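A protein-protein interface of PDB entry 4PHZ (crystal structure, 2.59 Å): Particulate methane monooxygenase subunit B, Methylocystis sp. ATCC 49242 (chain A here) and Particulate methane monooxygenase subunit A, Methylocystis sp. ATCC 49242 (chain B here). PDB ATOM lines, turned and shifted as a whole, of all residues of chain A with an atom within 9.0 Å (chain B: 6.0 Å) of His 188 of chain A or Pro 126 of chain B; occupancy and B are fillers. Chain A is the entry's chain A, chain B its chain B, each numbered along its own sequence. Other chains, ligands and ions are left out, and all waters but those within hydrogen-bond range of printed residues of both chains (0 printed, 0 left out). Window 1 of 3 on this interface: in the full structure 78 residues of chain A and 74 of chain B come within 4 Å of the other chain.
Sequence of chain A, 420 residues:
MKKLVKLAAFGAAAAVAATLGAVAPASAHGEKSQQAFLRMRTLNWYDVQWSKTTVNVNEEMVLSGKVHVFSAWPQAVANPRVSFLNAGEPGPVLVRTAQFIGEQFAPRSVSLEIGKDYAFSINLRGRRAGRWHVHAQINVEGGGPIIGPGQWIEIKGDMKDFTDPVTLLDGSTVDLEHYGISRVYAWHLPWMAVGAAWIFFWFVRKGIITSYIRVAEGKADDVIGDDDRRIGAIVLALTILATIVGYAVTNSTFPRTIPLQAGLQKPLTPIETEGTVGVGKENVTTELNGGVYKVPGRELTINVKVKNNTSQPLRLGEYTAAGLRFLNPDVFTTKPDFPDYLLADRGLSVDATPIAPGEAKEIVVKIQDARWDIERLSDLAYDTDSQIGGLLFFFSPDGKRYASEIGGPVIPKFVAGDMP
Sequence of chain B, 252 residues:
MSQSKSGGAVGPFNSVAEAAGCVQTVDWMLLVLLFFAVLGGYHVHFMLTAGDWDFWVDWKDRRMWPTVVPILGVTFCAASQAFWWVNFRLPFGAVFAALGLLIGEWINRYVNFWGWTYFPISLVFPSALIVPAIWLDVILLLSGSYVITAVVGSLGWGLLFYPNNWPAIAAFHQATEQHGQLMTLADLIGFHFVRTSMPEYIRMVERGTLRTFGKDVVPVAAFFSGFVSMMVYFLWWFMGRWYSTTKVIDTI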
ATOM      1  N   GLY A 180     -16.583 -25.787  -8.530  1.00  0.00           N
ATOM      2  CA  GLY A 180     -15.386 -25.319  -7.820  1.00  0.00           C
ATOM      3  C   GLY A 180     -14.240 -24.873  -8.706  1.00  0.00           C
ATOM      4  O   GLY A 180     -13.399 -24.083  -8.278  1.00  0.00           O
ATOM      5  N   ILE A 181     -14.210 -25.382  -9.935  1.00  0.00           N
ATOM      6  CA  ILE A 181     -13.100 -25.175 -10.858  1.00  0.00           C
ATOM      7  C   ILE A 181     -12.854 -23.707 -11.234  1.00  0.00           C
ATOM      8  O   ILE A 181     -11.707 -23.306 -11.475  1.00  0.00           O
ATOM      9  CB  ILE A 181     -13.246 -26.066 -12.120  1.00  0.00           C
ATOM     10  CG1 ILE A 181     -12.968 -27.534 -11.768  1.00  0.00           C
ATOM     11  CG2 ILE A 181     -12.305 -25.615 -13.230  1.00  0.00           C
ATOM     12  CD1 ILE A 181     -13.521 -28.538 -12.760  1.00  0.00           C
ATOM     13  N   SER A 182     -13.913 -22.899 -11.284  1.00  0.00           N
ATOM     14  CA  SER A 182     -13.742 -21.470 -11.584  1.00  0.00           C
ATOM     15  C   SER A 182     -13.011 -20.739 -10.478  1.00  0.00           C
ATOM     16  O   SER A 182     -12.072 -20.003 -10.748  1.00  0.00           O
ATOM     17  CB  SER A 182     -15.071 -20.789 -11.862  1.00  0.00           C
ATOM     18  OG  SER A 182     -15.201 -20.554 -13.254  1.00  0.00           O
ATOM     19  N   ARG A 183     -13.450 -20.962  -9.244  1.00  0.00           N
ATOM     20  CA  ARG A 183     -12.853 -20.374  -8.052  1.00  0.00           C
ATOM     21  C   ARG A 183     -11.336 -20.654  -7.943  1.00  0.00           C
ATOM     22  O   ARG A 183     -10.543 -19.787  -7.530  1.00  0.00           O
ATOM     23  CB  ARG A 183     -13.600 -20.904  -6.837  1.00  0.00           C
ATOM     24  CG  ARG A 183     -13.219 -20.281  -5.511  1.00  0.00           C
ATOM     25  CD  ARG A 183     -14.251 -20.656  -4.451  1.00  0.00           C
ATOM     26  NE  ARG A 183     -15.520 -19.946  -4.650  1.00  0.00           N
ATOM     27  CZ  ARG A 183     -15.781 -18.745  -4.137  1.00  0.00           C
ATOM     28  NH1 ARG A 183     -14.864 -18.138  -3.382  1.00  0.00           N
ATOM     29  NH2 ARG A 183     -16.952 -18.151  -4.370  1.00  0.00           N
ATOM     30  N   VAL A 184     -10.948 -21.865  -8.339  1.00  0.00           N
ATOM     31  CA  VAL A 184      -9.549 -22.316  -8.322  1.00  0.00           C
ATOM     32  C   VAL A 184      -8.691 -21.468  -9.263  1.00  0.00           C
ATOM     33  O   VAL A 184      -7.736 -20.842  -8.806  1.00  0.00           O
ATOM     34  CB  VAL A 184      -9.435 -23.837  -8.631  1.00  0.00           C
ATOM     35  CG1 VAL A 184      -8.022 -24.227  -9.051  1.00  0.00           C
ATOM     36  CG2 VAL A 184      -9.896 -24.654  -7.425  1.00  0.00           C
ATOM     37  N   TYR A 185      -9.050 -21.439 -10.553  1.00  0.00           N
ATOM     38  CA  TYR A 185      -8.443 -20.546 -11.542  1.00  0.00           C
ATOM     39  C   TYR A 185      -8.467 -19.082 -11.125  1.00  0.00           C
ATOM     40  O   TYR A 185      -7.470 -18.372 -11.295  1.00  0.00           O
ATOM     41  CB  TYR A 185      -9.200 -20.621 -12.837  1.00  0.00           C
ATOM     42  CG  TYR A 185      -9.080 -21.893 -13.608  1.00  0.00           C
ATOM     43  CD1 TYR A 185      -7.850 -22.553 -13.759  1.00  0.00           C
ATOM     44  CD2 TYR A 185     -10.199 -22.418 -14.254  1.00  0.00           C
ATOM     45  CE1 TYR A 185      -7.760 -23.718 -14.517  1.00  0.00           C
ATOM     46  CE2 TYR A 185     -10.120 -23.572 -15.010  1.00  0.00           C
ATOM     47  CZ  TYR A 185      -8.908 -24.216 -15.143  1.00  0.00           C
ATOM     48  OH  TYR A 185      -8.882 -25.358 -15.907  1.00  0.00           O
ATOM     49  N   ALA A 186      -9.611 -18.626 -10.614  1.00  0.00           N
ATOM     50  CA  ALA A 186      -9.754 -17.261 -10.115  1.00  0.00           C
ATOM     51  C   ALA A 186      -8.661 -16.899  -9.107  1.00  0.00           C
ATOM     52  O   ALA A 186      -8.197 -15.782  -9.084  1.00  0.00           O
ATOM     53  CB  ALA A 186     -11.134 -17.055  -9.509  1.00  0.00           C
ATOM     54  N   TRP A 187      -8.242 -17.859  -8.292  1.00  0.00           N
ATOM     55  CA  TRP A 187      -7.199 -17.636  -7.296  1.00  0.00           C
ATOM     56  C   TRP A 187      -5.816 -17.979  -7.779  1.00  0.00           C
ATOM     57  O   TRP A 187      -4.846 -17.333  -7.397  1.00  0.00           O
ATOM     58  CB  TRP A 187      -7.506 -18.476  -6.086  1.00  0.00           C
ATOM     59  CG  TRP A 187      -6.634 -18.193  -4.902  1.00  0.00           C
ATOM     60  CD1 TRP A 187      -5.675 -19.023  -4.330  1.00  0.00           C
ATOM     61  CD2 TRP A 187      -6.636 -16.985  -4.081  1.00  0.00           C
ATOM     62  NE1 TRP A 187      -5.103 -18.428  -3.237  1.00  0.00           N
ATOM     63  CE2 TRP A 187      -5.630 -17.200  -3.033  1.00  0.00           C
ATOM     64  CE3 TRP A 187      -7.343 -15.789  -4.106  1.00  0.00           C
ATOM     65  CZ2 TRP A 187      -5.359 -16.241  -2.067  1.00  0.00           C
ATOM     66  CZ3 TRP A 187      -7.064 -14.833  -3.124  1.00  0.00           C
ATOM     67  CH2 TRP A 187      -6.099 -15.056  -2.129  1.00  0.00           C
ATOM     68  N   HIS A 188      -5.706 -19.007  -8.614  1.00  0.00           N
ATOM     69  CA  HIS A 188      -4.398 -19.480  -9.060  1.00  0.00           C
ATOM     70  C   HIS A 188      -3.740 -18.610 -10.088  1.00  0.00           C
ATOM     71  O   HIS A 188      -2.548 -18.303  -9.966  1.00  0.00           O
ATOM     72  CB  HIS A 188      -4.431 -20.964  -9.481  1.00  0.00           C
ATOM     73  CG  HIS A 188      -4.143 -21.922  -8.334  1.00  0.00           C
ATOM     74  ND1 HIS A 188      -3.058 -22.717  -8.305  1.00  0.00           N
ATOM     75  CD2 HIS A 188      -4.822 -22.139  -7.123  1.00  0.00           C
ATOM     76  CE1 HIS A 188      -3.049 -23.419  -7.150  1.00  0.00           C
ATOM     77  NE2 HIS A 188      -4.129 -23.062  -6.429  1.00  0.00           N
ATOM     78  N   LEU A 189      -4.495 -18.182 -11.089  1.00  0.00           N
ATOM     79  CA  LEU A 189      -3.881 -17.476 -12.219  1.00  0.00           C
ATOM     80  C   LEU A 189      -3.447 -16.039 -11.892  1.00  0.00           C
ATOM     81  O   LEU A 189      -2.349 -15.643 -12.282  1.00  0.00           O
ATOM     82  CB  LEU A 189      -4.708 -17.606 -13.519  1.00  0.00           C
ATOM     83  CG  LEU A 189      -5.119 -19.044 -13.942  1.00  0.00           C
ATOM     84  CD1 LEU A 189      -5.636 -19.105 -15.376  1.00  0.00           C
ATOM     85  CD2 LEU A 189      -3.998 -20.081 -13.740  1.00  0.00           C
ATOM     86  N   PRO A 190      -4.282 -15.263 -11.149  1.00  0.00           N
ATOM     87  CA  PRO A 190      -3.759 -13.983 -10.622  1.00  0.00           C
ATOM     88  C   PRO A 190      -2.386 -14.105  -9.972  1.00  0.00           C
ATOM     89  O   PRO A 190      -1.458 -13.389 -10.364  1.00  0.00           O
ATOM     90  CB  PRO A 190      -4.819 -13.563  -9.598  1.00  0.00           C
ATOM     91  CG  PRO A 190      -6.091 -14.091 -10.190  1.00  0.00           C
ATOM     92  CD  PRO A 190      -5.742 -15.371 -10.928  1.00  0.00           C
ATOM     93  N   TRP A 191      -2.245 -15.023  -9.025  1.00  0.00           N
ATOM     94  CA  TRP A 191      -0.978 -15.187  -8.307  1.00  0.00           C
ATOM     95  C   TRP A 191       0.178 -15.613  -9.156  1.00  0.00           C
ATOM     96  O   TRP A 191       1.316 -15.162  -8.953  1.00  0.00           O
ATOM     97  CB  TRP A 191      -1.132 -16.141  -7.158  1.00  0.00           C
ATOM     98  CG  TRP A 191      -1.797 -15.496  -5.989  1.00  0.00           C
ATOM     99  CD1 TRP A 191      -2.992 -15.865  -5.398  1.00  0.00           C
ATOM    100  CD2 TRP A 191      -1.332 -14.332  -5.227  1.00  0.00           C
ATOM    101  NE1 TRP A 191      -3.289 -15.046  -4.335  1.00  0.00           N
ATOM    102  CE2 TRP A 191      -2.335 -14.104  -4.176  1.00  0.00           C
ATOM    103  CE3 TRP A 191      -0.220 -13.497  -5.288  1.00  0.00           C
ATOM    104  CZ2 TRP A 191      -2.215 -13.068  -3.247  1.00  0.00           C
ATOM    105  CZ3 TRP A 191      -0.100 -12.461  -4.334  1.00  0.00           C
ATOM    106  CH2 TRP A 191      -1.077 -12.254  -3.344  1.00  0.00           C
ATOM    107  N   MET A 192      -0.084 -16.476 -10.126  1.00  0.00           N
ATOM    108  CA  MET A 192       0.952 -16.782 -11.088  1.00  0.00           C
ATOM    109  C   MET A 192       1.369 -15.561 -11.891  1.00  0.00           C
ATOM    110  O   MET A 192       2.553 -15.342 -12.080  1.00  0.00           O
ATOM    111  CB  MET A 192       0.530 -17.913 -12.004  1.00  0.00           C
ATOM    112  CG  MET A 192       0.752 -19.280 -11.390  1.00  0.00           C
ATOM    113  SD  MET A 192      -0.100 -20.530 -12.366  1.00  0.00           S
ATOM    114  CE  MET A 192       1.109 -20.940 -13.622  1.00  0.00           C
ATOM    115  N   ALA A 193       0.396 -14.780 -12.365  1.00  0.00           N
ATOM    116  CA  ALA A 193       0.667 -13.518 -13.073  1.00  0.00           C
ATOM    117  C   ALA A 193       1.465 -12.546 -12.186  1.00  0.00           C
ATOM    118  O   ALA A 193       2.530 -12.051 -12.613  1.00  0.00           O
ATOM    119  CB  ALA A 193      -0.629 -12.873 -13.535  1.00  0.00           C
ATOM    120  N   VAL A 194       0.964 -12.306 -10.957  1.00  0.00           N
ATOM    121  CA  VAL A 194       1.667 -11.479  -9.969  1.00  0.00           C
ATOM    122  C   VAL A 194       3.099 -11.938  -9.764  1.00  0.00           C
ATOM    123  O   VAL A 194       4.006 -11.115  -9.762  1.00  0.00           O
ATOM    124  CB  VAL A 194       0.960 -11.433  -8.604  1.00  0.00           C
ATOM    125  CG1 VAL A 194       1.899 -10.911  -7.517  1.00  0.00           C
ATOM    126  CG2 VAL A 194      -0.288 -10.571  -8.675  1.00  0.00           C
ATOM    127  N   GLY A 195       3.298 -13.240  -9.601  1.00  0.00           N
ATOM    128  CA  GLY A 195       4.641 -13.810  -9.474  1.00  0.00           C
ATOM    129  C   GLY A 195       5.543 -13.504 -10.658  1.00  0.00           C
ATOM    130  O   GLY A 195       6.690 -13.123 -10.442  1.00  0.00           O
ATOM    131  N   ASP B  54       0.028 -33.228  -3.612  1.00  0.00           N
ATOM    132  CA  ASP B  54      -0.149 -32.096  -4.507  1.00  0.00           C
ATOM    133  C   ASP B  54      -1.101 -32.438  -5.658  1.00  0.00           C
ATOM    134  O   ASP B  54      -1.914 -31.586  -6.090  1.00  0.00           O
ATOM    135  CB  ASP B  54       1.195 -31.592  -5.035  1.00  0.00           C
ATOM    136  CG  ASP B  54       1.088 -30.207  -5.625  1.00  0.00           C
ATOM    137  OD1 ASP B  54       1.145 -29.202  -4.873  1.00  0.00           O
ATOM    138  OD2 ASP B  54       0.907 -30.135  -6.858  1.00  0.00           O
ATOM    139  N   PHE B  55      -1.000 -33.684  -6.132  1.00  0.00           N
ATOM    140  CA  PHE B  55      -1.860 -34.208  -7.196  1.00  0.00           C
ATOM    141  C   PHE B  55      -3.370 -34.176  -6.918  1.00  0.00           C
ATOM    142  O   PHE B  55      -4.128 -33.899  -7.844  1.00  0.00           O
ATOM    143  CB  PHE B  55      -1.536 -35.669  -7.454  1.00  0.00           C
ATOM    144  CG  PHE B  55      -0.227 -35.917  -8.113  1.00  0.00           C
ATOM    145  CD1 PHE B  55       0.694 -34.901  -8.319  1.00  0.00           C
ATOM    146  CD2 PHE B  55       0.101 -37.206  -8.499  1.00  0.00           C
ATOM    147  CE1 PHE B  55       1.910 -35.169  -8.939  1.00  0.00           C
ATOM    148  CE2 PHE B  55       1.307 -37.485  -9.100  1.00  0.00           C
ATOM    149  CZ  PHE B  55       2.216 -36.466  -9.325  1.00  0.00           C
ATOM    150  N   LYS B  60      -5.567 -33.221   0.341  1.00  0.00           N
ATOM    151  CA  LYS B  60      -5.315 -31.906   0.901  1.00  0.00           C
ATOM    152  C   LYS B  60      -5.991 -31.764   2.267  1.00  0.00           C
ATOM    153  O   LYS B  60      -6.998 -31.082   2.429  1.00  0.00           O
ATOM    154  CB  LYS B  60      -5.633 -30.795  -0.112  1.00  0.00           C
ATOM    155  CG  LYS B  60      -4.938 -31.024  -1.458  1.00  0.00           C
ATOM    156  CD  LYS B  60      -4.529 -29.758  -2.156  1.00  0.00           C
ATOM    157  CE  LYS B  60      -4.568 -29.954  -3.656  1.00  0.00           C
ATOM    158  NZ  LYS B  60      -3.500 -30.845  -4.175  1.00  0.00           N
ATOM    159  N   LEU B 102       4.789 -24.128 -10.114  1.00  0.00           N
ATOM    160  CA  LEU B 102       3.362 -23.900 -10.420  1.00  0.00           C
ATOM    161  C   LEU B 102       3.007 -23.992 -11.898  1.00  0.00           C
ATOM    162  O   LEU B 102       2.117 -24.763 -12.267  1.00  0.00           O
ATOM    163  CB  LEU B 102       2.875 -22.594  -9.827  1.00  0.00           C
ATOM    164  CG  LEU B 102       2.460 -22.931  -8.406  1.00  0.00           C
ATOM    165  CD1 LEU B 102       2.115 -21.704  -7.572  1.00  0.00           C
ATOM    166  CD2 LEU B 102       1.260 -23.850  -8.504  1.00  0.00           C
ATOM    167  N   GLU B 105       3.486 -27.682 -13.142  1.00  0.00           N
ATOM    168  CA  GLU B 105       2.365 -28.492 -12.643  1.00  0.00           C
ATOM    169  C   GLU B 105       1.053 -28.165 -13.382  1.00  0.00           C
ATOM    170  O   GLU B 105       0.378 -29.078 -13.891  1.00  0.00           O
ATOM    171  CB  GLU B 105       2.146 -28.270 -11.152  1.00  0.00           C
ATOM    172  CG  GLU B 105       3.228 -28.833 -10.265  1.00  0.00           C
ATOM    173  CD  GLU B 105       3.028 -28.434  -8.803  1.00  0.00           C
ATOM    174  OE1 GLU B 105       2.451 -27.339  -8.547  1.00  0.00           O
ATOM    175  OE2 GLU B 105       3.455 -29.209  -7.902  1.00  0.00           O
ATOM    176  N   TRP B 106       0.698 -26.872 -13.422  1.00  0.00           N
ATOM    177  CA  TRP B 106      -0.528 -26.444 -14.068  1.00  0.00           C
ATOM    178  C   TRP B 106      -0.582 -26.880 -15.488  1.00  0.00           C
ATOM    179  O   TRP B 106      -1.604 -27.415 -15.929  1.00  0.00           O
ATOM    180  CB  TRP B 106      -0.699 -24.960 -13.978  1.00  0.00           C
ATOM    181  CG  TRP B 106      -1.546 -24.538 -12.809  1.00  0.00           C
ATOM    182  CD1 TRP B 106      -1.161 -23.767 -11.704  1.00  0.00           C
ATOM    183  CD2 TRP B 106      -2.961 -24.830 -12.583  1.00  0.00           C
ATOM    184  NE1 TRP B 106      -2.211 -23.572 -10.838  1.00  0.00           N
ATOM    185  CE2 TRP B 106      -3.323 -24.171 -11.308  1.00  0.00           C
ATOM    186  CE3 TRP B 106      -3.932 -25.520 -13.280  1.00  0.00           C
ATOM    187  CZ2 TRP B 106      -4.605 -24.238 -10.784  1.00  0.00           C
ATOM    188  CZ3 TRP B 106      -5.222 -25.569 -12.740  1.00  0.00           C
ATOM    189  CH2 TRP B 106      -5.546 -24.947 -11.520  1.00  0.00           C
ATOM    190  N   ARG B 109      -1.264 -30.770 -15.175  1.00  0.00           N
ATOM    191  CA  ARG B 109      -2.605 -31.029 -14.701  1.00  0.00           C
ATOM    192  C   ARG B 109      -3.550 -30.822 -15.858  1.00  0.00           C
ATOM    193  O   ARG B 109      -4.330 -31.718 -16.173  1.00  0.00           O
ATOM    194  CB  ARG B 109      -2.984 -30.120 -13.521  1.00  0.00           C
ATOM    195  CG  ARG B 109      -2.000 -30.129 -12.347  1.00  0.00           C
ATOM    196  CD  ARG B 109      -1.585 -31.536 -11.923  1.00  0.00           C
ATOM    197  NE  ARG B 109      -0.414 -31.534 -11.049  1.00  0.00           N
ATOM    198  CZ  ARG B 109      -0.441 -31.294  -9.733  1.00  0.00           C
ATOM    199  NH1 ARG B 109      -1.584 -31.025  -9.087  1.00  0.00           N
ATOM    200  NH2 ARG B 109       0.699 -31.321  -9.053  1.00  0.00           N
ATOM    201  N   VAL B 124      -7.346 -32.386  -9.357  1.00  0.00           N
ATOM    202  CA  VAL B 124      -5.913 -32.403  -9.627  1.00  0.00           C
ATOM    203  C   VAL B 124      -5.186 -31.043  -9.589  1.00  0.00           C
ATOM    204  O   VAL B 124      -4.033 -30.903 -10.032  1.00  0.00           O
ATOM    205  CB  VAL B 124      -5.641 -33.124 -10.967  1.00  0.00           C
ATOM    206  CG1 VAL B 124      -6.173 -34.552 -10.914  1.00  0.00           C
ATOM    207  CG2 VAL B 124      -6.270 -32.368 -12.134  1.00  0.00           C
ATOM    208  N   PHE B 125      -5.836 -30.030  -9.040  1.00  0.00           N
ATOM    209  CA  PHE B 125      -5.182 -28.732  -8.994  1.00  0.00           C
ATOM    210  C   PHE B 125      -4.085 -28.739  -7.923  1.00  0.00           C
ATOM    211  O   PHE B 125      -4.266 -29.382  -6.880  1.00  0.00           O
ATOM    212  CB  PHE B 125      -6.193 -27.616  -8.772  1.00  0.00           C
ATOM    213  CG  PHE B 125      -6.882 -27.683  -7.463  1.00  0.00           C
ATOM    214  CD1 PHE B 125      -8.055 -28.408  -7.317  1.00  0.00           C
ATOM    215  CD2 PHE B 125      -6.365 -27.008  -6.368  1.00  0.00           C
ATOM    216  CE1 PHE B 125      -8.697 -28.465  -6.089  1.00  0.00           C
ATOM    217  CE2 PHE B 125      -7.003 -27.059  -5.138  1.00  0.00           C
ATOM    218  CZ  PHE B 125      -8.169 -27.792  -4.995  1.00  0.00           C
ATOM    219  N   PRO B 126      -2.938 -28.056  -8.196  1.00  0.00           N
ATOM    220  CA  PRO B 126      -1.748 -27.968  -7.339  1.00  0.00           C
ATOM    221  C   PRO B 126      -1.876 -27.058  -6.112  1.00  0.00           C
ATOM    222  O   PRO B 126      -2.827 -26.288  -5.987  1.00  0.00           O
ATOM    223  CB  PRO B 126      -0.709 -27.392  -8.277  1.00  0.00           C
ATOM    224  CG  PRO B 126      -1.510 -26.551  -9.214  1.00  0.00           C
ATOM    225  CD  PRO B 126      -2.669 -27.447  -9.515  1.00  0.00           C
ATOM    226  N   SER B 127      -0.915 -27.171  -5.198  1.00  0.00           N
ATOM    227  CA  SER B 127      -0.906 -26.378  -3.973  1.00  0.00           C
ATOM    228  C   SER B 127      -0.389 -24.980  -4.296  1.00  0.00           C
ATOM    229  O   SER B 127       0.493 -24.807  -5.157  1.00  0.00           O
ATOM    230  CB  SER B 127       0.000 -27.024  -2.908  1.00  0.00           C
ATOM    231  OG  SER B 127      -0.291 -28.401  -2.678  1.00  0.00           O
ATOM    232  N   ALA B 128      -0.913 -23.976  -3.602  1.00  0.00           N
ATOM    233  CA  ALA B 128      -0.547 -22.604  -3.941  1.00  0.00           C
ATOM    234  C   ALA B 128       0.671 -22.160  -3.136  1.00  0.00           C
ATOM    235  O   ALA B 128       0.661 -22.177  -1.904  1.00  0.00           O
ATOM    236  CB  ALA B 128      -1.736 -21.647  -3.763  1.00  0.00           C
ATOM    237  N   ILE B 130       2.805 -19.170  -4.209  1.00  0.00           N
ATOM    238  CA  ILE B 130       3.324 -17.876  -4.581  1.00  0.00           C
ATOM    239  C   ILE B 130       3.335 -16.852  -3.444  1.00  0.00           C
ATOM    240  O   ILE B 130       4.388 -16.252  -3.179  1.00  0.00           O
ATOM    241  CB  ILE B 130       2.803 -17.395  -5.943  1.00  0.00           C
ATOM    242  CG1 ILE B 130       3.798 -17.869  -6.997  1.00  0.00           C
ATOM    243  CG2 ILE B 130       2.733 -15.878  -6.005  1.00  0.00           C
ATOM    244  CD1 ILE B 130       3.164 -18.365  -8.267  1.00  0.00           C
ATOM    245  N   ASN B 165      -3.960 -21.081   0.628  1.00  0.00           N
ATOM    246  CA  ASN B 165      -4.572 -22.192  -0.079  1.00  0.00           C
ATOM    247  C   ASN B 165      -6.053 -22.245   0.166  1.00  0.00           C
ATOM    248  O   ASN B 165      -6.818 -22.605  -0.731  1.00  0.00           O
ATOM    249  CB  ASN B 165      -3.899 -23.528   0.256  1.00  0.00           C
ATOM    250  CG  ASN B 165      -2.837 -23.916  -0.770  1.00  0.00           C
ATOM    251  OD1 ASN B 165      -3.155 -24.330  -1.915  1.00  0.00           O
ATOM    252  ND2 ASN B 165      -1.566 -23.769  -0.377  1.00  0.00           N
ATOM    253  N   ALA B 168      -8.767 -21.598  -2.472  1.00  0.00           N
ATOM    254  CA  ALA B 168      -8.858 -22.635  -3.500  1.00  0.00           C
ATOM    255  C   ALA B 168      -9.470 -23.943  -2.972  1.00  0.00           C
ATOM    256  O   ALA B 168      -9.978 -24.748  -3.755  1.00  0.00           O
ATOM    257  CB  ALA B 168      -7.484 -22.903  -4.089  1.00  0.00           C
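ND1 of His 188 of chain A lies within hydrogen-bond range of NE1 of Trp 106 of chain B (2.8 Å).
O of Phe 125 of chain B is in hydrogen-bond range of NZ of Lys 60 of chain B (3.2 Å).
The side-chain amide oxygen (OD1) of Asn 165 of chain B lies within hydrogen-bond range of the backbone NH (N) of Ala 128 of chain B (2.8 Å).
Among the printed residues, pairs that only touch across the chains: His 188 of chain A with Pro 126 of chain B (3.1 Å), Trp 191 of chain A with Ile 130 of chain B (3.3 Å), Met 192 of chain A with Trp 106 of chain B (3.5 Å), Val 184 of chain A with Trp 106 of chain B (3.6 Å), Tyr 185 of chain A with Trp 106 of chain B (3.6 Å), Val 184 of chain A with Ala 168 of chain B (3.7 Å), His 188 of chain A with Ala 128 of chain B (3.9 Å), Val 184 of chain A with Phe 125 of chain B (3.9 Å), Met 192 of chain A with Ile 130 of chain B (3.9 Å) and Met 192 of chain A with Leu 102 of chain B (3.99 Å).
His 188 of chain A touches just these residues of chain B: Trp 106, Pro 126 and Ala 128.
Printed residues of chain B within 4 Å of Trp 191 of chain A: Ile 130.
Of the printed residues of chain A, Trp 106 of chain B touches Val 184, Tyr 185, His 188 and Met 192.
Of the printed residues of chain A, Phe 125 of chain B touches Val 184.
Ser 127 of chain B touches none of the printed residues of chain A.
Printed residues of chain A within 4 Å of Ile 130 of chain B: Trp 191 (3.3 Å) and Met 192 (3.9 Å).
The nearest residue of chain B that does not touch His 188 of chain A is Ala 168 of chain B (4.1 Å).
Of the 15 printed residues of chain B, 7 touch a printed residue of chain A.
Hydrophobic or aromatic side chains of chain B within 4 Å of the printed part of chain A: Trp 106, Phe 125, Ala 128 and Ile 130.
Of the 16 printed residues of chain A, 5 touch a printed residue of chain B.
Printed residues of chain A that touch a printed residue of chain B: Val 184, Tyr 185, His 188, Trp 191 and Met 192.
Among the printed residues, 11 pairs touch across the chains.
Among the printed residues, no Asp or Glu carboxylate lies within 4 Å of a Lys or Arg side-chain nitrogen of the other chain.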
